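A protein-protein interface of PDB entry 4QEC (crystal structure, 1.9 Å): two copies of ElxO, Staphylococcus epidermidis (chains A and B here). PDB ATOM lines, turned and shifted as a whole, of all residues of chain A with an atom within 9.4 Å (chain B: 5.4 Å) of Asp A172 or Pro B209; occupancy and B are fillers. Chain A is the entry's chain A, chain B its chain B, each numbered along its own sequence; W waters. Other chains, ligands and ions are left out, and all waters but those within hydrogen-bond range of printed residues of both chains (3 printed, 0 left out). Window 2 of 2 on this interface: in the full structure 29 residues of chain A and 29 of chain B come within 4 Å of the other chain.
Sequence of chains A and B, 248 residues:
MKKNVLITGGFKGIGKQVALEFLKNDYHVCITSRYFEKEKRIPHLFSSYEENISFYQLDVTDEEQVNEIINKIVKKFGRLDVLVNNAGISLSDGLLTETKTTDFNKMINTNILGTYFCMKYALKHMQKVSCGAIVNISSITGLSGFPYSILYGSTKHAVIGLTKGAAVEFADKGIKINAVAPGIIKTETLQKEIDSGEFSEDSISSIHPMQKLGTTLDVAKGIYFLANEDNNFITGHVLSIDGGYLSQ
OD1 of Asp B242 sits at hydrogen-bond distance from N of Gly B244.
The side-chain amino group (NZ) of Lys A176 lies within hydrogen-bond range of the backbone carbonyl oxygen (O) of Gly A174 (3.2 Å).
OG of Ser B247 is in hydrogen-bond range of O of Gly B244, 2.6 Å away.
The side-chain amide oxygen (OE1) of Gln B211 lies close to the backbone carbonyl oxygen (O) of His B208.
The backbone NH (N) of Tyr B245 lies close to the side-chain carboxylate (OD2) of Asp B242, 3.4 Å away.
The backbone NH (N) of Gly A236 sits at hydrogen-bond distance from the backbone carbonyl oxygen (O) of Ile A177, at 2.8 Å.
Of chain B, only Pro B209 comes within 4 Å of Asp A172.
Of chain A, only Thr A235 comes within 4 Å of Gly B244.
Of the printed residues of chain B, Ala A171 touches Pro B209 and Met B210.
Of the printed residues of chain B, Thr A235 touches Gly B243 (3.8 Å) and Gly B244 (3.3 Å).
Tyr B245 touches none of the printed residues of chain A.
The nearest residue of chain B that does not touch Asp A172 is Gln B211 (4.1 Å).
The nearest residue of chain A that does not touch Pro B209 is Val A168 (4.7 Å).
The nearest printed residue of chain A that does not touch His B208 is Ala A171 (6.2 Å).
Among the printed residues, merely in contact across the chains: Thr A235 with Gly B244 (3.3 Å), Val A168 with Ser B247 (3.4 Å), Gly A236 with Ser B247 (3.4 Å), Ala A171 with Pro B209 (3.5 Å), Ala A171 with Met B210 (3.5 Å), Lys A176 with Met B210 (3.5 Å), Asp A172 with Pro B209 (3.7 Å), Thr A235 with Gly B243 (3.8 Å), Phe A233 with Met B210 (3.9 Å) and Phe A233 with His B208 (3.9 Å).
The backbone carbonyl oxygen of Phe A233 is in hydrogen-bond range of the backbone NH of Gly B243 (2.8 Å).
N of Asp B242 sits at hydrogen-bond distance from O of Phe A233 (3.4 Å).
O of Asn A232 lies close to SD of Met B210 (3.6 Å).
Water W2 lies within hydrogen-bond range of O of Ala A171 (2.6 Å), N of Gly A174 (3.2 Å) and O of Met B210 (3.3 Å).
Water W3 lies within hydrogen-bond range of the side-chain carboxylate of Asp B242 (2.7 Å) and the backbone NH of Thr A235 (3.2 Å).
Water W1 bridges the backbone carbonyl oxygen (O) of Thr A235 (2.9 Å) and the side-chain carboxylate (OD1) of Asp B242 (2.9 Å).
Hydrophobic or aromatic side chains of chain B within 4 Å of the printed part of chain A: His B208, Pro B209 and Met B210.
Hydrophobic or aromatic side chains of chain A that line the printed part of chain B: Val A168, Ala A171 and Phe A233.
Among the printed residues, 13 pairs touch across the chains.
No position is printed for both chains.
Of the 13 pairs that touch across the chains among the printed residues, none has its exchanged pair printed and touching as well.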
ATOM      1  N   GLN A 127      22.630  13.184  -3.634  1.00  0.00           N
ATOM      2  CA  GLN A 127      24.044  12.858  -3.329  1.00  0.00           C
ATOM      3  C   GLN A 127      24.194  12.096  -2.017  1.00  0.00           C
ATOM      4  O   GLN A 127      24.973  11.149  -1.920  1.00  0.00           O
ATOM      5  CB  GLN A 127      24.860  14.144  -3.170  1.00  0.00           C
ATOM      6  CG  GLN A 127      25.723  14.544  -4.344  1.00  0.00           C
ATOM      7  CD  GLN A 127      26.543  15.792  -4.052  1.00  0.00           C
ATOM      8  OE1 GLN A 127      26.156  16.641  -3.241  1.00  0.00           O
ATOM      9  NE2 GLN A 127      27.686  15.906  -4.709  1.00  0.00           N
ATOM     10  N   VAL A 129      22.111  10.136  -0.478  1.00  0.00           N
ATOM     11  CA  VAL A 129      21.571   8.777  -0.464  1.00  0.00           C
ATOM     12  C   VAL A 129      22.107   7.910  -1.611  1.00  0.00           C
ATOM     13  O   VAL A 129      21.757   6.727  -1.720  1.00  0.00           O
ATOM     14  CB  VAL A 129      20.020   8.756  -0.389  1.00  0.00           C
ATOM     15  CG1 VAL A 129      19.557   9.313   0.951  1.00  0.00           C
ATOM     16  CG2 VAL A 129      19.389   9.536  -1.536  1.00  0.00           C
ATOM     17  N   SER A 130      22.959   8.505  -2.450  1.00  0.00           N
ATOM     18  CA  SER A 130      23.560   7.819  -3.598  1.00  0.00           C
ATOM     19  C   SER A 130      22.532   7.105  -4.488  1.00  0.00           C
ATOM     20  O   SER A 130      22.743   5.962  -4.898  1.00  0.00           O
ATOM     21  CB  SER A 130      24.653   6.837  -3.146  1.00  0.00           C
ATOM     22  OG  SER A 130      25.671   7.528  -2.451  1.00  0.00           O
ATOM     23  N   CYS A 131      21.424   7.785  -4.776  1.00  0.00           N
ATOM     24  CA  CYS A 131      20.416   7.279  -5.710  1.00  0.00           C
ATOM     25  C   CYS A 131      19.445   8.387  -6.094  1.00  0.00           C
ATOM     26  O   CYS A 131      19.371   9.426  -5.433  1.00  0.00           O
ATOM     27  CB  CYS A 131      19.657   6.089  -5.127  1.00  0.00           C
ATOM     28  SG  CYS A 131      18.635   6.542  -3.725  1.00  0.00           S
ATOM     29  N   LYS A 164      24.151  16.064 -19.843  1.00  0.00           N
ATOM     30  CA  LYS A 164      25.302  15.203 -20.085  1.00  0.00           C
ATOM     31  C   LYS A 164      26.404  15.492 -19.063  1.00  0.00           C
ATOM     32  O   LYS A 164      26.988  14.574 -18.503  1.00  0.00           O
ATOM     33  CB  LYS A 164      25.843  15.402 -21.497  1.00  0.00           C
ATOM     34  CG  LYS A 164      24.970  14.841 -22.607  1.00  0.00           C
ATOM     35  CD  LYS A 164      25.702  15.009 -23.927  1.00  0.00           C
ATOM     36  CE  LYS A 164      25.004  14.304 -25.068  1.00  0.00           C
ATOM     37  NZ  LYS A 164      25.873  14.381 -26.278  1.00  0.00           N
ATOM     38  N   GLY A 165      26.675  16.773 -18.826  1.00  0.00           N
ATOM     39  CA  GLY A 165      27.672  17.164 -17.823  1.00  0.00           C
ATOM     40  C   GLY A 165      27.372  16.619 -16.433  1.00  0.00           C
ATOM     41  O   GLY A 165      28.249  16.026 -15.785  1.00  0.00           O
ATOM     42  N   ALA A 166      26.143  16.832 -15.963  1.00  0.00           N
ATOM     43  CA  ALA A 166      25.721  16.324 -14.656  1.00  0.00           C
ATOM     44  C   ALA A 166      25.771  14.801 -14.592  1.00  0.00           C
ATOM     45  O   ALA A 166      26.249  14.221 -13.607  1.00  0.00           O
ATOM     46  CB  ALA A 166      24.322  16.827 -14.303  1.00  0.00           C
ATOM     47  N   ALA A 167      25.291  14.149 -15.652  1.00  0.00           N
ATOM     48  CA  ALA A 167      25.324  12.689 -15.734  1.00  0.00           C
ATOM     49  C   ALA A 167      26.720  12.130 -15.474  1.00  0.00           C
ATOM     50  O   ALA A 167      26.886  11.214 -14.647  1.00  0.00           O
ATOM     51  CB  ALA A 167      24.831  12.219 -17.090  1.00  0.00           C
ATOM     52  N   VAL A 168      27.709  12.669 -16.186  1.00  0.00           N
ATOM     53  CA  VAL A 168      29.090  12.199 -16.055  1.00  0.00           C
ATOM     54  C   VAL A 168      29.588  12.475 -14.638  1.00  0.00           C
ATOM     55  O   VAL A 168      30.197  11.609 -14.012  1.00  0.00           O
ATOM     56  CB  VAL A 168      30.044  12.801 -17.121  1.00  0.00           C
ATOM     57  CG1 VAL A 168      31.467  12.294 -16.910  1.00  0.00           C
ATOM     58  CG2 VAL A 168      29.590  12.419 -18.528  1.00  0.00           C
ATOM     59  N   GLU A 169      29.293  13.665 -14.130  1.00  0.00           N
ATOM     60  CA  GLU A 169      29.717  14.046 -12.792  1.00  0.00           C
ATOM     61  C   GLU A 169      29.094  13.180 -11.679  1.00  0.00           C
ATOM     62  O   GLU A 169      29.761  12.866 -10.685  1.00  0.00           O
ATOM     63  CB  GLU A 169      29.420  15.524 -12.566  1.00  0.00           C
ATOM     64  CG  GLU A 169      30.205  16.156 -11.431  1.00  0.00           C
ATOM     65  CD  GLU A 169      29.994  17.654 -11.381  1.00  0.00           C
ATOM     66  OE1 GLU A 169      30.600  18.389 -12.201  1.00  0.00           O
ATOM     67  OE2 GLU A 169      29.199  18.079 -10.530  1.00  0.00           O
ATOM     68  N   PHE A 170      27.832  12.781 -11.848  1.00  0.00           N
ATOM     69  CA  PHE A 170      27.137  12.019 -10.805  1.00  0.00           C
ATOM     70  C   PHE A 170      26.964  10.526 -11.091  1.00  0.00           C
ATOM     71  O   PHE A 170      26.285   9.821 -10.333  1.00  0.00           O
ATOM     72  CB  PHE A 170      25.790  12.679 -10.461  1.00  0.00           C
ATOM     73  CG  PHE A 170      25.943  13.997  -9.759  1.00  0.00           C
ATOM     74  CD1 PHE A 170      25.957  14.061  -8.366  1.00  0.00           C
ATOM     75  CD2 PHE A 170      26.133  15.167 -10.484  1.00  0.00           C
ATOM     76  CE1 PHE A 170      26.135  15.274  -7.711  1.00  0.00           C
ATOM     77  CE2 PHE A 170      26.311  16.382  -9.839  1.00  0.00           C
ATOM     78  CZ  PHE A 170      26.308  16.438  -8.450  1.00  0.00           C
ATOM     79  N   ALA A 171      27.594  10.049 -12.165  1.00  0.00           N
ATOM     80  CA  ALA A 171      27.458   8.654 -12.593  1.00  0.00           C
ATOM     81  C   ALA A 171      27.941   7.671 -11.544  1.00  0.00           C
ATOM     82  O   ALA A 171      27.314   6.636 -11.348  1.00  0.00           O
ATOM     83  CB  ALA A 171      28.182   8.419 -13.908  1.00  0.00           C
ATOM     84  N   ASP A 172      29.048   7.995 -10.871  1.00  0.00           N
ATOM     85  CA  ASP A 172      29.602   7.099  -9.854  1.00  0.00           C
ATOM     86  C   ASP A 172      28.905   7.236  -8.494  1.00  0.00           C
ATOM     87  O   ASP A 172      29.223   6.505  -7.553  1.00  0.00           O
ATOM     88  CB  ASP A 172      31.129   7.265  -9.733  1.00  0.00           C
ATOM     89  CG  ASP A 172      31.545   8.577  -9.071  1.00  0.00           C
ATOM     90  OD1 ASP A 172      30.746   9.544  -9.023  1.00  0.00           O
ATOM     91  OD2 ASP A 172      32.702   8.644  -8.603  1.00  0.00           O
ATOM     92  N   LYS A 173      27.947   8.162  -8.405  1.00  0.00           N
ATOM     93  CA  LYS A 173      27.127   8.318  -7.207  1.00  0.00           C
ATOM     94  C   LYS A 173      25.752   7.656  -7.339  1.00  0.00           C
ATOM     95  O   LYS A 173      24.876   7.872  -6.507  1.00  0.00           O
ATOM     96  CB  LYS A 173      27.003   9.799  -6.833  1.00  0.00           C
ATOM     97  CG  LYS A 173      28.315  10.390  -6.333  1.00  0.00           C
ATOM     98  CD  LYS A 173      28.214  11.887  -6.074  1.00  0.00           C
ATOM     99  CE  LYS A 173      29.590  12.512  -5.880  1.00  0.00           C
ATOM    100  NZ  LYS A 173      30.355  12.600  -7.157  1.00  0.00           N
ATOM    101  N   GLY A 174      25.577   6.852  -8.389  1.00  0.00           N
ATOM    102  CA  GLY A 174      24.352   6.078  -8.623  1.00  0.00           C
ATOM    103  C   GLY A 174      23.109   6.876  -8.995  1.00  0.00           C
ATOM    104  O   GLY A 174      21.986   6.403  -8.817  1.00  0.00           O
ATOM    105  N   ILE A 175      23.305   8.089  -9.494  1.00  0.00           N
ATOM    106  CA  ILE A 175      22.193   8.942  -9.908  1.00  0.00           C
ATOM    107  C   ILE A 175      22.112   8.904 -11.436  1.00  0.00           C
ATOM    108  O   ILE A 175      23.131   9.004 -12.107  1.00  0.00           O
ATOM    109  CB  ILE A 175      22.368  10.376  -9.344  1.00  0.00           C
ATOM    110  CG1 ILE A 175      22.357  10.330  -7.802  1.00  0.00           C
ATOM    111  CG2 ILE A 175      21.279  11.322  -9.857  1.00  0.00           C
ATOM    112  CD1 ILE A 175      22.950  11.553  -7.136  1.00  0.00           C
ATOM    113  N   LYS A 176      20.915   8.701 -11.977  1.00  0.00           N
ATOM    114  CA  LYS A 176      20.703   8.739 -13.429  1.00  0.00           C
ATOM    115  C   LYS A 176      20.176  10.109 -13.844  1.00  0.00           C
ATOM    116  O   LYS A 176      19.279  10.660 -13.207  1.00  0.00           O
ATOM    117  CB  LYS A 176      19.721   7.653 -13.892  1.00  0.00           C
ATOM    118  CG  LYS A 176      20.213   6.219 -13.706  1.00  0.00           C
ATOM    119  CD  LYS A 176      19.934   5.704 -12.303  1.00  0.00           C
ATOM    120  CE  LYS A 176      20.777   4.468 -12.012  1.00  0.00           C
ATOM    121  NZ  LYS A 176      20.732   4.066 -10.573  1.00  0.00           N
ATOM    122  N   ILE A 177      20.751  10.660 -14.909  1.00  0.00           N
ATOM    123  CA  ILE A 177      20.360  11.965 -15.412  1.00  0.00           C
ATOM    124  C   ILE A 177      20.282  11.906 -16.937  1.00  0.00           C
ATOM    125  O   ILE A 177      21.294  11.732 -17.626  1.00  0.00           O
ATOM    126  CB  ILE A 177      21.341  13.063 -14.955  1.00  0.00           C
ATOM    127  CG1 ILE A 177      21.468  13.073 -13.417  1.00  0.00           C
ATOM    128  CG2 ILE A 177      20.895  14.425 -15.475  1.00  0.00           C
ATOM    129  CD1 ILE A 177      22.536  14.013 -12.877  1.00  0.00           C
ATOM    130  N   ASN A 232      18.886   1.115 -14.362  1.00  0.00           N
ATOM    131  CA  ASN A 232      20.150   0.986 -13.635  1.00  0.00           C
ATOM    132  C   ASN A 232      21.387   1.406 -14.423  1.00  0.00           C
ATOM    133  O   ASN A 232      22.462   1.530 -13.835  1.00  0.00           O
ATOM    134  CB  ASN A 232      20.354  -0.459 -13.158  1.00  0.00           C
ATOM    135  CG  ASN A 232      19.297  -0.901 -12.166  1.00  0.00           C
ATOM    136  OD1 ASN A 232      18.626  -1.915 -12.373  1.00  0.00           O
ATOM    137  ND2 ASN A 232      19.142  -0.146 -11.090  1.00  0.00           N
ATOM    138  N   PHE A 233      21.264   1.602 -15.741  1.00  0.00           N
ATOM    139  CA  PHE A 233      22.466   1.739 -16.578  1.00  0.00           C
ATOM    140  C   PHE A 233      22.332   2.769 -17.697  1.00  0.00           C
ATOM    141  O   PHE A 233      23.218   2.878 -18.544  1.00  0.00           O
ATOM    142  CB  PHE A 233      22.851   0.359 -17.163  1.00  0.00           C
ATOM    143  CG  PHE A 233      24.316   0.203 -17.502  1.00  0.00           C
ATOM    144  CD1 PHE A 233      25.306   0.425 -16.541  1.00  0.00           C
ATOM    145  CD2 PHE A 233      24.708  -0.219 -18.778  1.00  0.00           C
ATOM    146  CE1 PHE A 233      26.652   0.256 -16.852  1.00  0.00           C
ATOM    147  CE2 PHE A 233      26.053  -0.394 -19.093  1.00  0.00           C
ATOM    148  CZ  PHE A 233      27.028  -0.152 -18.129  1.00  0.00           C
ATOM    149  N   THR A 235      22.287   6.603 -18.515  1.00  0.00           N
ATOM    150  CA  THR A 235      22.505   7.966 -18.023  1.00  0.00           C
ATOM    151  C   THR A 235      23.261   8.796 -19.051  1.00  0.00           C
ATOM    152  O   THR A 235      24.007   8.251 -19.881  1.00  0.00           O
ATOM    153  CB  THR A 235      23.204   7.976 -16.633  1.00  0.00           C
ATOM    154  OG1 THR A 235      23.056   9.270 -16.027  1.00  0.00           O
ATOM    155  CG2 THR A 235      24.693   7.601 -16.738  1.00  0.00           C
ATOM    156  N   GLY A 236      23.052  10.109 -19.010  1.00  0.00           N
ATOM    157  CA  GLY A 236      23.657  11.015 -19.977  1.00  0.00           C
ATOM    158  C   GLY A 236      23.029  10.957 -21.363  1.00  0.00           C
ATOM    159  O   GLY A 236      23.583  11.503 -22.321  1.00  0.00           O
ATOM    160  N   SER B 206      35.546   0.137 -15.390  1.00  0.00           N
ATOM    161  CA  SER B 206      36.050   1.509 -15.281  1.00  0.00           C
ATOM    162  C   SER B 206      35.892   2.350 -16.553  1.00  0.00           C
ATOM    163  O   SER B 206      35.978   3.576 -16.496  1.00  0.00           O
ATOM    164  CB  SER B 206      37.520   1.501 -14.837  1.00  0.00           C
ATOM    165  OG  SER B 206      38.358   1.019 -15.875  1.00  0.00           O
ATOM    166  N   ILE B 207      35.646   1.716 -17.697  1.00  0.00           N
ATOM    167  CA  ILE B 207      35.393   2.505 -18.915  1.00  0.00           C
ATOM    168  C   ILE B 207      34.019   3.197 -18.909  1.00  0.00           C
ATOM    169  O   ILE B 207      33.817   4.176 -19.629  1.00  0.00           O
ATOM    170  CB  ILE B 207      35.631   1.717 -20.230  1.00  0.00           C
ATOM    171  CG1 ILE B 207      34.496   0.740 -20.515  1.00  0.00           C
ATOM    172  CG2 ILE B 207      36.985   1.016 -20.214  1.00  0.00           C
ATOM    173  CD1 ILE B 207      34.252   0.579 -21.995  1.00  0.00           C
ATOM    174  N   HIS B 208      33.089   2.700 -18.088  1.00  0.00           N
ATOM    175  CA  HIS B 208      31.778   3.344 -17.916  1.00  0.00           C
ATOM    176  C   HIS B 208      31.837   4.340 -16.760  1.00  0.00           C
ATOM    177  O   HIS B 208      32.341   4.006 -15.675  1.00  0.00           O
ATOM    178  CB  HIS B 208      30.671   2.333 -17.621  1.00  0.00           C
ATOM    179  CG  HIS B 208      30.677   1.134 -18.514  1.00  0.00           C
ATOM    180  ND1 HIS B 208      30.270   1.185 -19.832  1.00  0.00           N
ATOM    181  CD2 HIS B 208      31.002  -0.156 -18.272  1.00  0.00           C
ATOM    182  CE1 HIS B 208      30.366  -0.019 -20.368  1.00  0.00           C
ATOM    183  NE2 HIS B 208      30.810  -0.851 -19.443  1.00  0.00           N
ATOM    184  N   PRO B 209      31.332   5.567 -16.986  1.00  0.00           N
ATOM    185  CA  PRO B 209      31.216   6.554 -15.913  1.00  0.00           C
ATOM    186  C   PRO B 209      30.538   5.990 -14.654  1.00  0.00           C
ATOM    187  O   PRO B 209      30.952   6.320 -13.543  1.00  0.00           O
ATOM    188  CB  PRO B 209      30.390   7.663 -16.562  1.00  0.00           C
ATOM    189  CG  PRO B 209      30.858   7.642 -17.990  1.00  0.00           C
ATOM    190  CD  PRO B 209      31.160   6.191 -18.313  1.00  0.00           C
ATOM    191  N   MET B 210      29.539   5.122 -14.816  1.00  0.00           N
ATOM    192  CA  MET B 210      28.877   4.507 -13.655  1.00  0.00           C
ATOM    193  C   MET B 210      29.749   3.507 -12.880  1.00  0.00           C
ATOM    194  O   MET B 210      29.343   3.039 -11.824  1.00  0.00           O
ATOM    195  CB  MET B 210      27.535   3.862 -14.047  1.00  0.00           C
ATOM    196  CG  MET B 210      26.447   4.862 -14.406  1.00  0.00           C
ATOM    197  SD  MET B 210      24.812   4.103 -14.610  1.00  0.00           S
ATOM    198  CE  MET B 210      24.193   4.190 -12.933  1.00  0.00           C
ATOM    199  N   GLN B 211      30.925   3.174 -13.410  1.00  0.00           N
ATOM    200  CA  GLN B 211      31.891   2.308 -12.716  1.00  0.00           C
ATOM    201  C   GLN B 211      31.332   0.926 -12.358  1.00  0.00           C
ATOM    202  O   GLN B 211      31.574   0.423 -11.262  1.00  0.00           O
ATOM    203  CB  GLN B 211      32.439   3.009 -11.453  1.00  0.00           C
ATOM    204  CG  GLN B 211      33.158   4.327 -11.718  1.00  0.00           C
ATOM    205  CD  GLN B 211      34.453   4.154 -12.496  1.00  0.00           C
ATOM    206  OE1 GLN B 211      34.603   4.687 -13.596  1.00  0.00           O
ATOM    207  NE2 GLN B 211      35.391   3.400 -11.931  1.00  0.00           N
ATOM    208  N   ASP B 242      24.628   2.188 -21.531  1.00  0.00           N
ATOM    209  CA  ASP B 242      26.092   2.177 -21.486  1.00  0.00           C
ATOM    210  C   ASP B 242      26.725   2.827 -20.251  1.00  0.00           C
ATOM    211  O   ASP B 242      27.916   3.186 -20.269  1.00  0.00           O
ATOM    212  CB  ASP B 242      26.616   2.868 -22.747  1.00  0.00           C
ATOM    213  CG  ASP B 242      26.345   4.370 -22.762  1.00  0.00           C
ATOM    214  OD1 ASP B 242      25.609   4.891 -21.893  1.00  0.00           O
ATOM    215  OD2 ASP B 242      26.871   5.035 -23.673  1.00  0.00           O
ATOM    216  N   GLY B 243      25.941   2.991 -19.191  1.00  0.00           N
ATOM    217  CA  GLY B 243      26.441   3.610 -17.952  1.00  0.00           C
ATOM    218  C   GLY B 243      27.079   4.973 -18.163  1.00  0.00           C
ATOM    219  O   GLY B 243      27.992   5.365 -17.418  1.00  0.00           O
ATOM    220  N   GLY B 244      26.610   5.688 -19.188  1.00  0.00           N
ATOM    221  CA  GLY B 244      27.080   7.042 -19.486  1.00  0.00           C
ATOM    222  C   GLY B 244      28.227   7.116 -20.480  1.00  0.00           C
ATOM    223  O   GLY B 244      28.697   8.206 -20.801  1.00  0.00           O
ATOM    224  N   TYR B 245      28.679   5.970 -20.984  1.00  0.00           N
ATOM    225  CA  TYR B 245      29.884   5.949 -21.822  1.00  0.00           C
ATOM    226  C   TYR B 245      29.883   6.994 -22.939  1.00  0.00           C
ATOM    227  O   TYR B 245      30.856   7.752 -23.092  1.00  0.00           O
ATOM    228  CB  TYR B 245      30.160   4.562 -22.409  1.00  0.00           C
ATOM    229  CG  TYR B 245      31.428   4.555 -23.228  1.00  0.00           C
ATOM    230  CD1 TYR B 245      32.651   4.229 -22.644  1.00  0.00           C
ATOM    231  CD2 TYR B 245      31.413   4.920 -24.582  1.00  0.00           C
ATOM    232  CE1 TYR B 245      33.828   4.250 -23.380  1.00  0.00           C
ATOM    233  CE2 TYR B 245      32.582   4.946 -25.326  1.00  0.00           C
ATOM    234  CZ  TYR B 245      33.785   4.607 -24.722  1.00  0.00           C
ATOM    235  OH  TYR B 245      34.953   4.633 -25.457  1.00  0.00           O
ATOM    236  N   SER B 247      28.132   9.698 -23.310  1.00  0.00           N
ATOM    237  CA  SER B 247      27.876  11.089 -22.911  1.00  0.00           C
ATOM    238  C   SER B 247      29.162  11.847 -22.603  1.00  0.00           C
ATOM    239  O   SER B 247      29.144  13.068 -22.439  1.00  0.00           O
ATOM    240  CB  SER B 247      26.947  11.145 -21.710  1.00  0.00           C
ATOM    241  OG  SER B 247      27.585  10.588 -20.572  1.00  0.00           O
ATOM    242  N   GLN B 248      30.267  11.115 -22.482  1.00  0.00           N
ATOM    243  CA  GLN B 248      31.595  11.718 -22.415  1.00  0.00           C
ATOM    244  C   GLN B 248      32.198  11.731 -23.818  1.00  0.00           C
ATOM    245  O   GLN B 248      33.215  12.377 -24.057  1.00  0.00           O
ATOM    246  CB  GLN B 248      32.508  10.971 -21.431  1.00  0.00           C
ATOM    247  CG  GLN B 248      32.070   9.562 -21.077  1.00  0.00           C
ATOM    248  CD  GLN B 248      33.200   8.678 -20.580  1.00  0.00           C
ATOM    249  OE1 GLN B 248      33.883   9.003 -19.606  1.00  0.00           O
ATOM    250  NE2 GLN B 248      33.385   7.536 -21.235  1.00  0.00           N
HETATM  251  O   HOH W   1      25.242   7.710 -22.410  1.00  0.00           O
HETATM  252  O   HOH W   2      27.104   4.512  -9.856  1.00  0.00           O
HETATM  253  O   HOH W   3      23.044   5.296 -21.320  1.00  0.00           O
